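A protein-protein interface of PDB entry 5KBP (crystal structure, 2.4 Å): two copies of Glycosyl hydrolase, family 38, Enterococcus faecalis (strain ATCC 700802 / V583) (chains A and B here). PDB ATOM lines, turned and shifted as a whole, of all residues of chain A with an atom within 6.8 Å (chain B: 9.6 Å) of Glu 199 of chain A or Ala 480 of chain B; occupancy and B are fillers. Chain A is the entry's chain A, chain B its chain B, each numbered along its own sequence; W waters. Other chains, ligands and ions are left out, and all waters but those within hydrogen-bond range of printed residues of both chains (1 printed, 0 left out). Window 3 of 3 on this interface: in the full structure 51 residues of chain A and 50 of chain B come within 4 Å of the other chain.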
ATOM      1  N   SER A 195      13.302 -19.796  -8.236  1.00  0.00           N
ATOM      2  CA  SER A 195      14.668 -19.308  -8.131  1.00  0.00           C
ATOM      3  C   SER A 195      15.624 -20.348  -7.562  1.00  0.00           C
ATOM      4  O   SER A 195      16.740 -19.991  -7.166  1.00  0.00           O
ATOM      5  CB  SER A 195      14.718 -18.042  -7.269  1.00  0.00           C
ATOM      6  OG  SER A 195      14.161 -18.280  -5.988  1.00  0.00           O
ATOM      7  N   ASN A 196      15.221 -21.620  -7.510  1.00  0.00           N
ATOM      8  CA  ASN A 196      16.072 -22.639  -6.902  1.00  0.00           C
ATOM      9  C   ASN A 196      17.363 -22.838  -7.685  1.00  0.00           C
ATOM     10  O   ASN A 196      18.389 -23.207  -7.103  1.00  0.00           O
ATOM     11  CB  ASN A 196      15.312 -23.961  -6.785  1.00  0.00           C
ATOM     12  CG  ASN A 196      14.905 -24.518  -8.134  1.00  0.00           C
ATOM     13  OD1 ASN A 196      14.568 -23.772  -9.052  1.00  0.00           O
ATOM     14  ND2 ASN A 196      14.938 -25.840  -8.262  1.00  0.00           N
ATOM     15  N   GLY A 197      17.337 -22.596  -8.993  1.00  0.00           N
ATOM     16  CA  GLY A 197      18.522 -22.770  -9.809  1.00  0.00           C
ATOM     17  C   GLY A 197      19.192 -21.470 -10.202  1.00  0.00           C
ATOM     18  O   GLY A 197      19.905 -21.415 -11.208  1.00  0.00           O
ATOM     19  N   ASN A 198      18.982 -20.419  -9.412  1.00  0.00           N
ATOM     20  CA  ASN A 198      19.543 -19.116  -9.739  1.00  0.00           C
ATOM     21  C   ASN A 198      21.032 -19.082  -9.419  1.00  0.00           C
ATOM     22  O   ASN A 198      21.459 -19.530  -8.350  1.00  0.00           O
ATOM     23  CB  ASN A 198      18.811 -18.014  -8.974  1.00  0.00           C
ATOM     24  CG  ASN A 198      19.200 -16.626  -9.441  1.00  0.00           C
ATOM     25  OD1 ASN A 198      19.403 -16.393 -10.632  1.00  0.00           O
ATOM     26  ND2 ASN A 198      19.317 -15.694  -8.501  1.00  0.00           N
ATOM     27  N   GLU A 199      21.820 -18.553 -10.359  1.00  0.00           N
ATOM     28  CA  GLU A 199      23.264 -18.368 -10.205  1.00  0.00           C
ATOM     29  C   GLU A 199      23.952 -19.689  -9.842  1.00  0.00           C
ATOM     30  O   GLU A 199      24.398 -19.914  -8.715  1.00  0.00           O
ATOM     31  CB  GLU A 199      23.567 -17.280  -9.167  1.00  0.00           C
ATOM     32  CG  GLU A 199      22.870 -15.959  -9.447  1.00  0.00           C
ATOM     33  CD  GLU A 199      23.449 -14.809  -8.647  1.00  0.00           C
ATOM     34  OE1 GLU A 199      24.685 -14.772  -8.468  1.00  0.00           O
ATOM     35  OE2 GLU A 199      22.671 -13.944  -8.196  1.00  0.00           O
ATOM     36  N   ILE A 200      24.024 -20.560 -10.842  1.00  0.00           N
ATOM     37  CA  ILE A 200      24.687 -21.853 -10.697  1.00  0.00           C
ATOM     38  C   ILE A 200      26.195 -21.628 -10.683  1.00  0.00           C
ATOM     39  O   ILE A 200      26.740 -21.033 -11.625  1.00  0.00           O
ATOM     40  CB  ILE A 200      24.277 -22.818 -11.819  1.00  0.00           C
ATOM     41  CG1 ILE A 200      22.768 -23.079 -11.773  1.00  0.00           C
ATOM     42  CG2 ILE A 200      25.057 -24.118 -11.709  1.00  0.00           C
ATOM     43  CD1 ILE A 200      22.262 -23.928 -12.918  1.00  0.00           C
ATOM     44  N   PRO A 201      26.901 -22.070  -9.643  1.00  0.00           N
ATOM     45  CA  PRO A 201      28.350 -21.844  -9.586  1.00  0.00           C
ATOM     46  C   PRO A 201      29.082 -22.559 -10.713  1.00  0.00           C
ATOM     47  O   PRO A 201      28.801 -23.717 -11.030  1.00  0.00           O
ATOM     48  CB  PRO A 201      28.744 -22.413  -8.219  1.00  0.00           C
ATOM     49  CG  PRO A 201      27.488 -22.382  -7.417  1.00  0.00           C
ATOM     50  CD  PRO A 201      26.382 -22.647  -8.394  1.00  0.00           C
ATOM     51  N   SER A 202      30.033 -21.849 -11.319  1.00  0.00           N
ATOM     52  CA  SER A 202      30.918 -22.409 -12.329  1.00  0.00           C
ATOM     53  C   SER A 202      32.305 -22.715 -11.773  1.00  0.00           C
ATOM     54  O   SER A 202      33.271 -22.795 -12.538  1.00  0.00           O
ATOM     55  CB  SER A 202      31.022 -21.465 -13.527  1.00  0.00           C
ATOM     56  OG  SER A 202      31.573 -20.217 -13.148  1.00  0.00           O
ATOM     57  N   PHE A 210      26.603 -26.286  -3.679  1.00  0.00           N
ATOM     58  CA  PHE A 210      25.368 -25.816  -4.298  1.00  0.00           C
ATOM     59  C   PHE A 210      24.465 -26.986  -4.668  1.00  0.00           C
ATOM     60  O   PHE A 210      23.316 -27.068  -4.217  1.00  0.00           O
ATOM     61  CB  PHE A 210      25.695 -24.972  -5.532  1.00  0.00           C
ATOM     62  CG  PHE A 210      24.484 -24.463  -6.265  1.00  0.00           C
ATOM     63  CD1 PHE A 210      23.886 -23.268  -5.900  1.00  0.00           C
ATOM     64  CD2 PHE A 210      23.956 -25.168  -7.336  1.00  0.00           C
ATOM     65  CE1 PHE A 210      22.779 -22.793  -6.577  1.00  0.00           C
ATOM     66  CE2 PHE A 210      22.847 -24.699  -8.018  1.00  0.00           C
ATOM     67  CZ  PHE A 210      22.258 -23.509  -7.638  1.00  0.00           C
ATOM     68  N   MET A 230      15.029 -23.859 -11.844  1.00  0.00           N
ATOM     69  CA  MET A 230      14.667 -22.583 -12.453  1.00  0.00           C
ATOM     70  C   MET A 230      15.846 -21.624 -12.325  1.00  0.00           C
ATOM     71  O   MET A 230      16.123 -21.104 -11.238  1.00  0.00           O
ATOM     72  CB  MET A 230      13.409 -22.019 -11.801  1.00  0.00           C
ATOM     73  CG  MET A 230      12.174 -22.877 -12.031  1.00  0.00           C
ATOM     74  SD  MET A 230      11.776 -23.052 -13.784  1.00  0.00           S
ATOM     75  CE  MET A 230      11.470 -21.343 -14.221  1.00  0.00           C
ATOM     76  N   ASN A 231      16.534 -21.384 -13.441  1.00  0.00           N
ATOM     77  CA  ASN A 231      17.763 -20.590 -13.459  1.00  0.00           C
ATOM     78  C   ASN A 231      17.404 -19.123 -13.698  1.00  0.00           C
ATOM     79  O   ASN A 231      17.510 -18.588 -14.804  1.00  0.00           O
ATOM     80  CB  ASN A 231      18.720 -21.136 -14.513  1.00  0.00           C
ATOM     81  CG  ASN A 231      19.947 -20.269 -14.699  1.00  0.00           C
ATOM     82  OD1 ASN A 231      20.211 -19.784 -15.798  1.00  0.00           O
ATOM     83  ND2 ASN A 231      20.701 -20.065 -13.626  1.00  0.00           N
ATOM     84  N   GLY A 232      16.973 -18.469 -12.628  1.00  0.00           N
ATOM     85  CA  GLY A 232      16.603 -17.069 -12.703  1.00  0.00           C
ATOM     86  C   GLY A 232      15.819 -16.653 -11.479  1.00  0.00           C
ATOM     87  O   GLY A 232      15.543 -17.456 -10.583  1.00  0.00           O
ATOM     88  N   VAL A 233      15.458 -15.368 -11.465  1.00  0.00           N
ATOM     89  CA  VAL A 233      14.718 -14.768 -10.358  1.00  0.00           C
ATOM     90  C   VAL A 233      14.247 -13.380 -10.795  1.00  0.00           C
ATOM     91  O   VAL A 233      14.403 -13.006 -11.963  1.00  0.00           O
ATOM     92  CB  VAL A 233      15.580 -14.723  -9.076  1.00  0.00           C
ATOM     93  CG1 VAL A 233      16.650 -13.650  -9.173  1.00  0.00           C
ATOM     94  CG2 VAL A 233      14.722 -14.562  -7.816  1.00  0.00           C
ATOM     95  N   HIS A 235      14.008  -9.912 -11.953  1.00  0.00           N
ATOM     96  CA  HIS A 235      14.914  -8.948 -12.582  1.00  0.00           C
ATOM     97  C   HIS A 235      16.350  -9.464 -12.604  1.00  0.00           C
ATOM     98  O   HIS A 235      17.308  -8.705 -12.430  1.00  0.00           O
ATOM     99  CB  HIS A 235      14.835  -7.584 -11.891  1.00  0.00           C
ATOM    100  CG  HIS A 235      13.478  -6.953 -11.946  1.00  0.00           C
ATOM    101  ND1 HIS A 235      12.909  -6.317 -10.865  1.00  0.00           N
ATOM    102  CD2 HIS A 235      12.580  -6.855 -12.956  1.00  0.00           C
ATOM    103  CE1 HIS A 235      11.717  -5.858 -11.203  1.00  0.00           C
ATOM    104  NE2 HIS A 235      11.494  -6.171 -12.467  1.00  0.00           N
ATOM    105  N   GLN A 236      16.504 -10.758 -12.822  1.00  0.00           N
ATOM    106  CA  GLN A 236      17.832 -11.358 -12.820  1.00  0.00           C
ATOM    107  C   GLN A 236      18.456 -11.258 -14.205  1.00  0.00           C
ATOM    108  O   GLN A 236      17.830 -11.673 -15.188  1.00  0.00           O
ATOM    109  CB  GLN A 236      17.767 -12.819 -12.398  1.00  0.00           C
ATOM    110  CG  GLN A 236      19.117 -13.517 -12.330  1.00  0.00           C
ATOM    111  CD  GLN A 236      19.949 -13.086 -11.135  1.00  0.00           C
ATOM    112  OE1 GLN A 236      19.483 -12.341 -10.272  1.00  0.00           O
ATOM    113  NE2 GLN A 236      21.188 -13.561 -11.078  1.00  0.00           N
ATOM    114  N   PRO A 237      19.665 -10.714 -14.325  1.00  0.00           N
ATOM    115  CA  PRO A 237      20.378 -10.798 -15.602  1.00  0.00           C
ATOM    116  C   PRO A 237      20.648 -12.251 -15.958  1.00  0.00           C
ATOM    117  O   PRO A 237      20.834 -13.102 -15.085  1.00  0.00           O
ATOM    118  CB  PRO A 237      21.681 -10.035 -15.336  1.00  0.00           C
ATOM    119  CG  PRO A 237      21.389  -9.171 -14.148  1.00  0.00           C
ATOM    120  CD  PRO A 237      20.412  -9.944 -13.317  1.00  0.00           C
ATOM    121  N   GLN A 239      22.431 -15.533 -16.828  1.00  0.00           N
ATOM    122  CA  GLN A 239      23.733 -16.030 -16.395  1.00  0.00           C
ATOM    123  C   GLN A 239      24.601 -16.305 -17.616  1.00  0.00           C
ATOM    124  O   GLN A 239      24.357 -17.259 -18.361  1.00  0.00           O
ATOM    125  CB  GLN A 239      23.557 -17.286 -15.546  1.00  0.00           C
ATOM    126  CG  GLN A 239      24.857 -17.875 -15.032  1.00  0.00           C
ATOM    127  CD  GLN A 239      24.633 -19.050 -14.104  1.00  0.00           C
ATOM    128  OE1 GLN A 239      23.547 -19.219 -13.548  1.00  0.00           O
ATOM    129  NE2 GLN A 239      25.660 -19.873 -13.933  1.00  0.00           N
ATOM    130  N   ILE A 242      26.291 -19.842 -17.953  1.00  0.00           N
ATOM    131  CA  ILE A 242      25.412 -20.966 -17.646  1.00  0.00           C
ATOM    132  C   ILE A 242      25.870 -22.227 -18.367  1.00  0.00           C
ATOM    133  O   ILE A 242      25.708 -23.338 -17.849  1.00  0.00           O
ATOM    134  CB  ILE A 242      23.951 -20.610 -17.987  1.00  0.00           C
ATOM    135  CG1 ILE A 242      23.002 -21.714 -17.515  1.00  0.00           C
ATOM    136  CG2 ILE A 242      23.785 -20.351 -19.481  1.00  0.00           C
ATOM    137  CD1 ILE A 242      23.029 -21.941 -16.018  1.00  0.00           C
ATOM    138  N   ALA A 245      28.828 -23.703 -16.279  1.00  0.00           N
ATOM    139  CA  ALA A 245      28.410 -24.268 -15.000  1.00  0.00           C
ATOM    140  C   ALA A 245      27.690 -25.599 -15.180  1.00  0.00           C
ATOM    141  O   ALA A 245      27.815 -26.499 -14.341  1.00  0.00           O
ATOM    142  CB  ALA A 245      27.518 -23.276 -14.258  1.00  0.00           C
ATOM    143  N   ASP B 475      21.778  -2.129  -4.162  1.00  0.00           N
ATOM    144  CA  ASP B 475      22.517  -2.083  -5.411  1.00  0.00           C
ATOM    145  C   ASP B 475      21.848  -2.999  -6.426  1.00  0.00           C
ATOM    146  O   ASP B 475      21.312  -4.055  -6.075  1.00  0.00           O
ATOM    147  CB  ASP B 475      23.978  -2.511  -5.221  1.00  0.00           C
ATOM    148  CG  ASP B 475      24.743  -1.583  -4.305  1.00  0.00           C
ATOM    149  OD1 ASP B 475      24.322  -0.419  -4.146  1.00  0.00           O
ATOM    150  OD2 ASP B 475      25.773  -2.018  -3.750  1.00  0.00           O
ATOM    151  N   LEU B 476      21.874  -2.583  -7.688  1.00  0.00           N
ATOM    152  CA  LEU B 476      21.364  -3.414  -8.772  1.00  0.00           C
ATOM    153  C   LEU B 476      22.519  -3.804  -9.685  1.00  0.00           C
ATOM    154  O   LEU B 476      22.753  -3.146 -10.708  1.00  0.00           O
ATOM    155  CB  LEU B 476      20.272  -2.684  -9.557  1.00  0.00           C
ATOM    156  CG  LEU B 476      18.983  -2.378  -8.794  1.00  0.00           C
ATOM    157  CD1 LEU B 476      17.984  -1.677  -9.699  1.00  0.00           C
ATOM    158  CD2 LEU B 476      18.391  -3.655  -8.214  1.00  0.00           C
ATOM    159  N   PRO B 477      23.268  -4.852  -9.344  1.00  0.00           N
ATOM    160  CA  PRO B 477      24.425  -5.230 -10.161  1.00  0.00           C
ATOM    161  C   PRO B 477      24.007  -5.671 -11.554  1.00  0.00           C
ATOM    162  O   PRO B 477      22.877  -6.101 -11.791  1.00  0.00           O
ATOM    163  CB  PRO B 477      25.055  -6.391  -9.378  1.00  0.00           C
ATOM    164  CG  PRO B 477      24.499  -6.275  -7.993  1.00  0.00           C
ATOM    165  CD  PRO B 477      23.121  -5.718  -8.164  1.00  0.00           C
ATOM    166  N   LYS B 478      24.949  -5.557 -12.489  1.00  0.00           N
ATOM    167  CA  LYS B 478      24.722  -5.983 -13.863  1.00  0.00           C
ATOM    168  C   LYS B 478      24.888  -7.484 -14.054  1.00  0.00           C
ATOM    169  O   LYS B 478      24.655  -7.979 -15.162  1.00  0.00           O
ATOM    170  CB  LYS B 478      25.674  -5.242 -14.806  1.00  0.00           C
ATOM    171  CG  LYS B 478      25.561  -3.732 -14.730  1.00  0.00           C
ATOM    172  CD  LYS B 478      24.153  -3.274 -15.074  1.00  0.00           C
ATOM    173  CE  LYS B 478      23.997  -1.777 -14.878  1.00  0.00           C
ATOM    174  NZ  LYS B 478      22.630  -1.314 -15.238  1.00  0.00           N
ATOM    175  N   ASP B 479      25.277  -8.218 -13.007  1.00  0.00           N
ATOM    176  CA  ASP B 479      25.536  -9.645 -13.145  1.00  0.00           C
ATOM    177  C   ASP B 479      25.019 -10.466 -11.968  1.00  0.00           C
ATOM    178  O   ASP B 479      25.316 -11.666 -11.897  1.00  0.00           O
ATOM    179  CB  ASP B 479      27.040  -9.892 -13.320  1.00  0.00           C
ATOM    180  CG  ASP B 479      27.859  -9.335 -12.171  1.00  0.00           C
ATOM    181  OD1 ASP B 479      27.327  -8.497 -11.414  1.00  0.00           O
ATOM    182  OD2 ASP B 479      29.035  -9.731 -12.028  1.00  0.00           O
ATOM    183  N   ALA B 480      24.263  -9.874 -11.047  1.00  0.00           N
ATOM    184  CA  ALA B 480      23.780 -10.608  -9.887  1.00  0.00           C
ATOM    185  C   ALA B 480      22.448 -10.029  -9.433  1.00  0.00           C
ATOM    186  O   ALA B 480      21.970  -9.019  -9.955  1.00  0.00           O
ATOM    187  CB  ALA B 480      24.802 -10.580  -8.744  1.00  0.00           C
ATOM    188  N   PHE B 481      21.857 -10.691  -8.441  1.00  0.00           N
ATOM    189  CA  PHE B 481      20.582 -10.288  -7.868  1.00  0.00           C
ATOM    190  C   PHE B 481      20.730  -8.960  -7.120  1.00  0.00           C
ATOM    191  O   PHE B 481      21.837  -8.474  -6.867  1.00  0.00           O
ATOM    192  CB  PHE B 481      20.064 -11.386  -6.936  1.00  0.00           C
ATOM    193  CG  PHE B 481      18.650 -11.182  -6.463  1.00  0.00           C
ATOM    194  CD1 PHE B 481      17.630 -10.944  -7.367  1.00  0.00           C
ATOM    195  CD2 PHE B 481      18.341 -11.249  -5.114  1.00  0.00           C
ATOM    196  CE1 PHE B 481      16.328 -10.764  -6.935  1.00  0.00           C
ATOM    197  CE2 PHE B 481      17.041 -11.070  -4.675  1.00  0.00           C
ATOM    198  CZ  PHE B 481      16.034 -10.827  -5.587  1.00  0.00           C
ATOM    199  N   ARG B 482      19.588  -8.364  -6.776  1.00  0.00           N
ATOM    200  CA  ARG B 482      19.595  -7.144  -5.981  1.00  0.00           C
ATOM    201  C   ARG B 482      20.237  -7.406  -4.624  1.00  0.00           C
ATOM    202  O   ARG B 482      20.096  -8.489  -4.049  1.00  0.00           O
ATOM    203  CB  ARG B 482      18.170  -6.615  -5.802  1.00  0.00           C
ATOM    204  CG  ARG B 482      17.247  -7.562  -5.051  1.00  0.00           C
ATOM    205  CD  ARG B 482      15.969  -6.861  -4.626  1.00  0.00           C
ATOM    206  NE  ARG B 482      14.792  -7.371  -5.322  1.00  0.00           N
ATOM    207  CZ  ARG B 482      13.958  -8.270  -4.810  1.00  0.00           C
ATOM    208  NH1 ARG B 482      14.173  -8.754  -3.595  1.00  0.00           N
ATOM    209  NH2 ARG B 482      12.908  -8.681  -5.508  1.00  0.00           N
ATOM    210  N   GLN B 483      20.956  -6.409  -4.114  1.00  0.00           N
ATOM    211  CA  GLN B 483      21.645  -6.524  -2.829  1.00  0.00           C
ATOM    212  C   GLN B 483      21.191  -5.410  -1.899  1.00  0.00           C
ATOM    213  O   GLN B 483      21.639  -4.258  -2.043  1.00  0.00           O
ATOM    214  CB  GLN B 483      23.161  -6.483  -3.015  1.00  0.00           C
ATOM    215  CG  GLN B 483      23.930  -6.704  -1.727  1.00  0.00           C
ATOM    216  CD  GLN B 483      23.483  -7.957  -0.994  1.00  0.00           C
ATOM    217  OE1 GLN B 483      22.849  -7.884   0.059  1.00  0.00           O
ATOM    218  NE2 GLN B 483      23.813  -9.116  -1.551  1.00  0.00           N
HETATM  219  O   HOH W   1      14.463  -7.167  -8.283  1.00  0.00           O
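Glu 199 of chain A touches Ala 480 of chain B.
Val 233 of chain A touches Phe 481 of chain B (CG1 to CD1, 3.4 Å).
Ala 480 of chain B touches Gln 236 of chain A (C to OE1, 3.9 Å).
Lys 478 of chain B touches Pro 237 of chain A (O to CB, 3.6 Å).
O of Ala 480 of chain B touches CD of Pro 237 of chain A, at 3.8 Å.
The side-chain carboxylate (OE2) of Glu 199 of chain A sits at hydrogen-bond distance from the backbone NH (N) of Phe 481 of chain B (3.4 Å).
N of Phe 481 of chain B lies close to OE1 of Gln 236 of chain A.
Of the 9 printed residues of chain B, 3 touch a printed residue of chain A.
Hydrophobic or aromatic side chains of chain B within 4 Å of the printed part of chain A: Phe 481.
Asn 196 of chain A touches none of the printed residues of chain B.
Ile 200 of chain A touches none of the printed residues of chain B.
Of the printed residues of chain B, Val 233 of chain A touches Phe 481.
Of the printed residues of chain B, Gln 236 of chain A touches Ala 480 and Phe 481.
Ile 242 of chain A touches none of the printed residues of chain B.
Ala 480 of chain B touches just these residues of chain A: Glu 199, Gln 236 and Pro 237.
Of the printed residues of chain A, Phe 481 of chain B touches Glu 199, Val 233 and Gln 236.
The nearest residue of chain B that does not touch Glu 199 of chain A is Asp 479 of chain B (4.7 Å).
The nearest residue of chain A that does not touch Ala 480 of chain B is His 235 of chain A (5.3 Å).
The nearest printed residue of chain B that does not touch Gln 236 of chain A is Asp 479 of chain B (4.6 Å).
NE2 of Gln 236 of chain A sits close to OD1 of Asn 198 of chain A (3.4 Å).
The side-chain amide nitrogen (NE2) of Gln 236 of chain A lies within hydrogen-bond range of the side-chain carboxylate (OE2) of Glu 199 of chain A (3.3 Å).
No position is printed for both chains.
Water W1 lies within hydrogen-bond range of NE of Arg 482 of chain B (3.0 Å) and ND1 of His 235 of chain A (3.1 Å).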
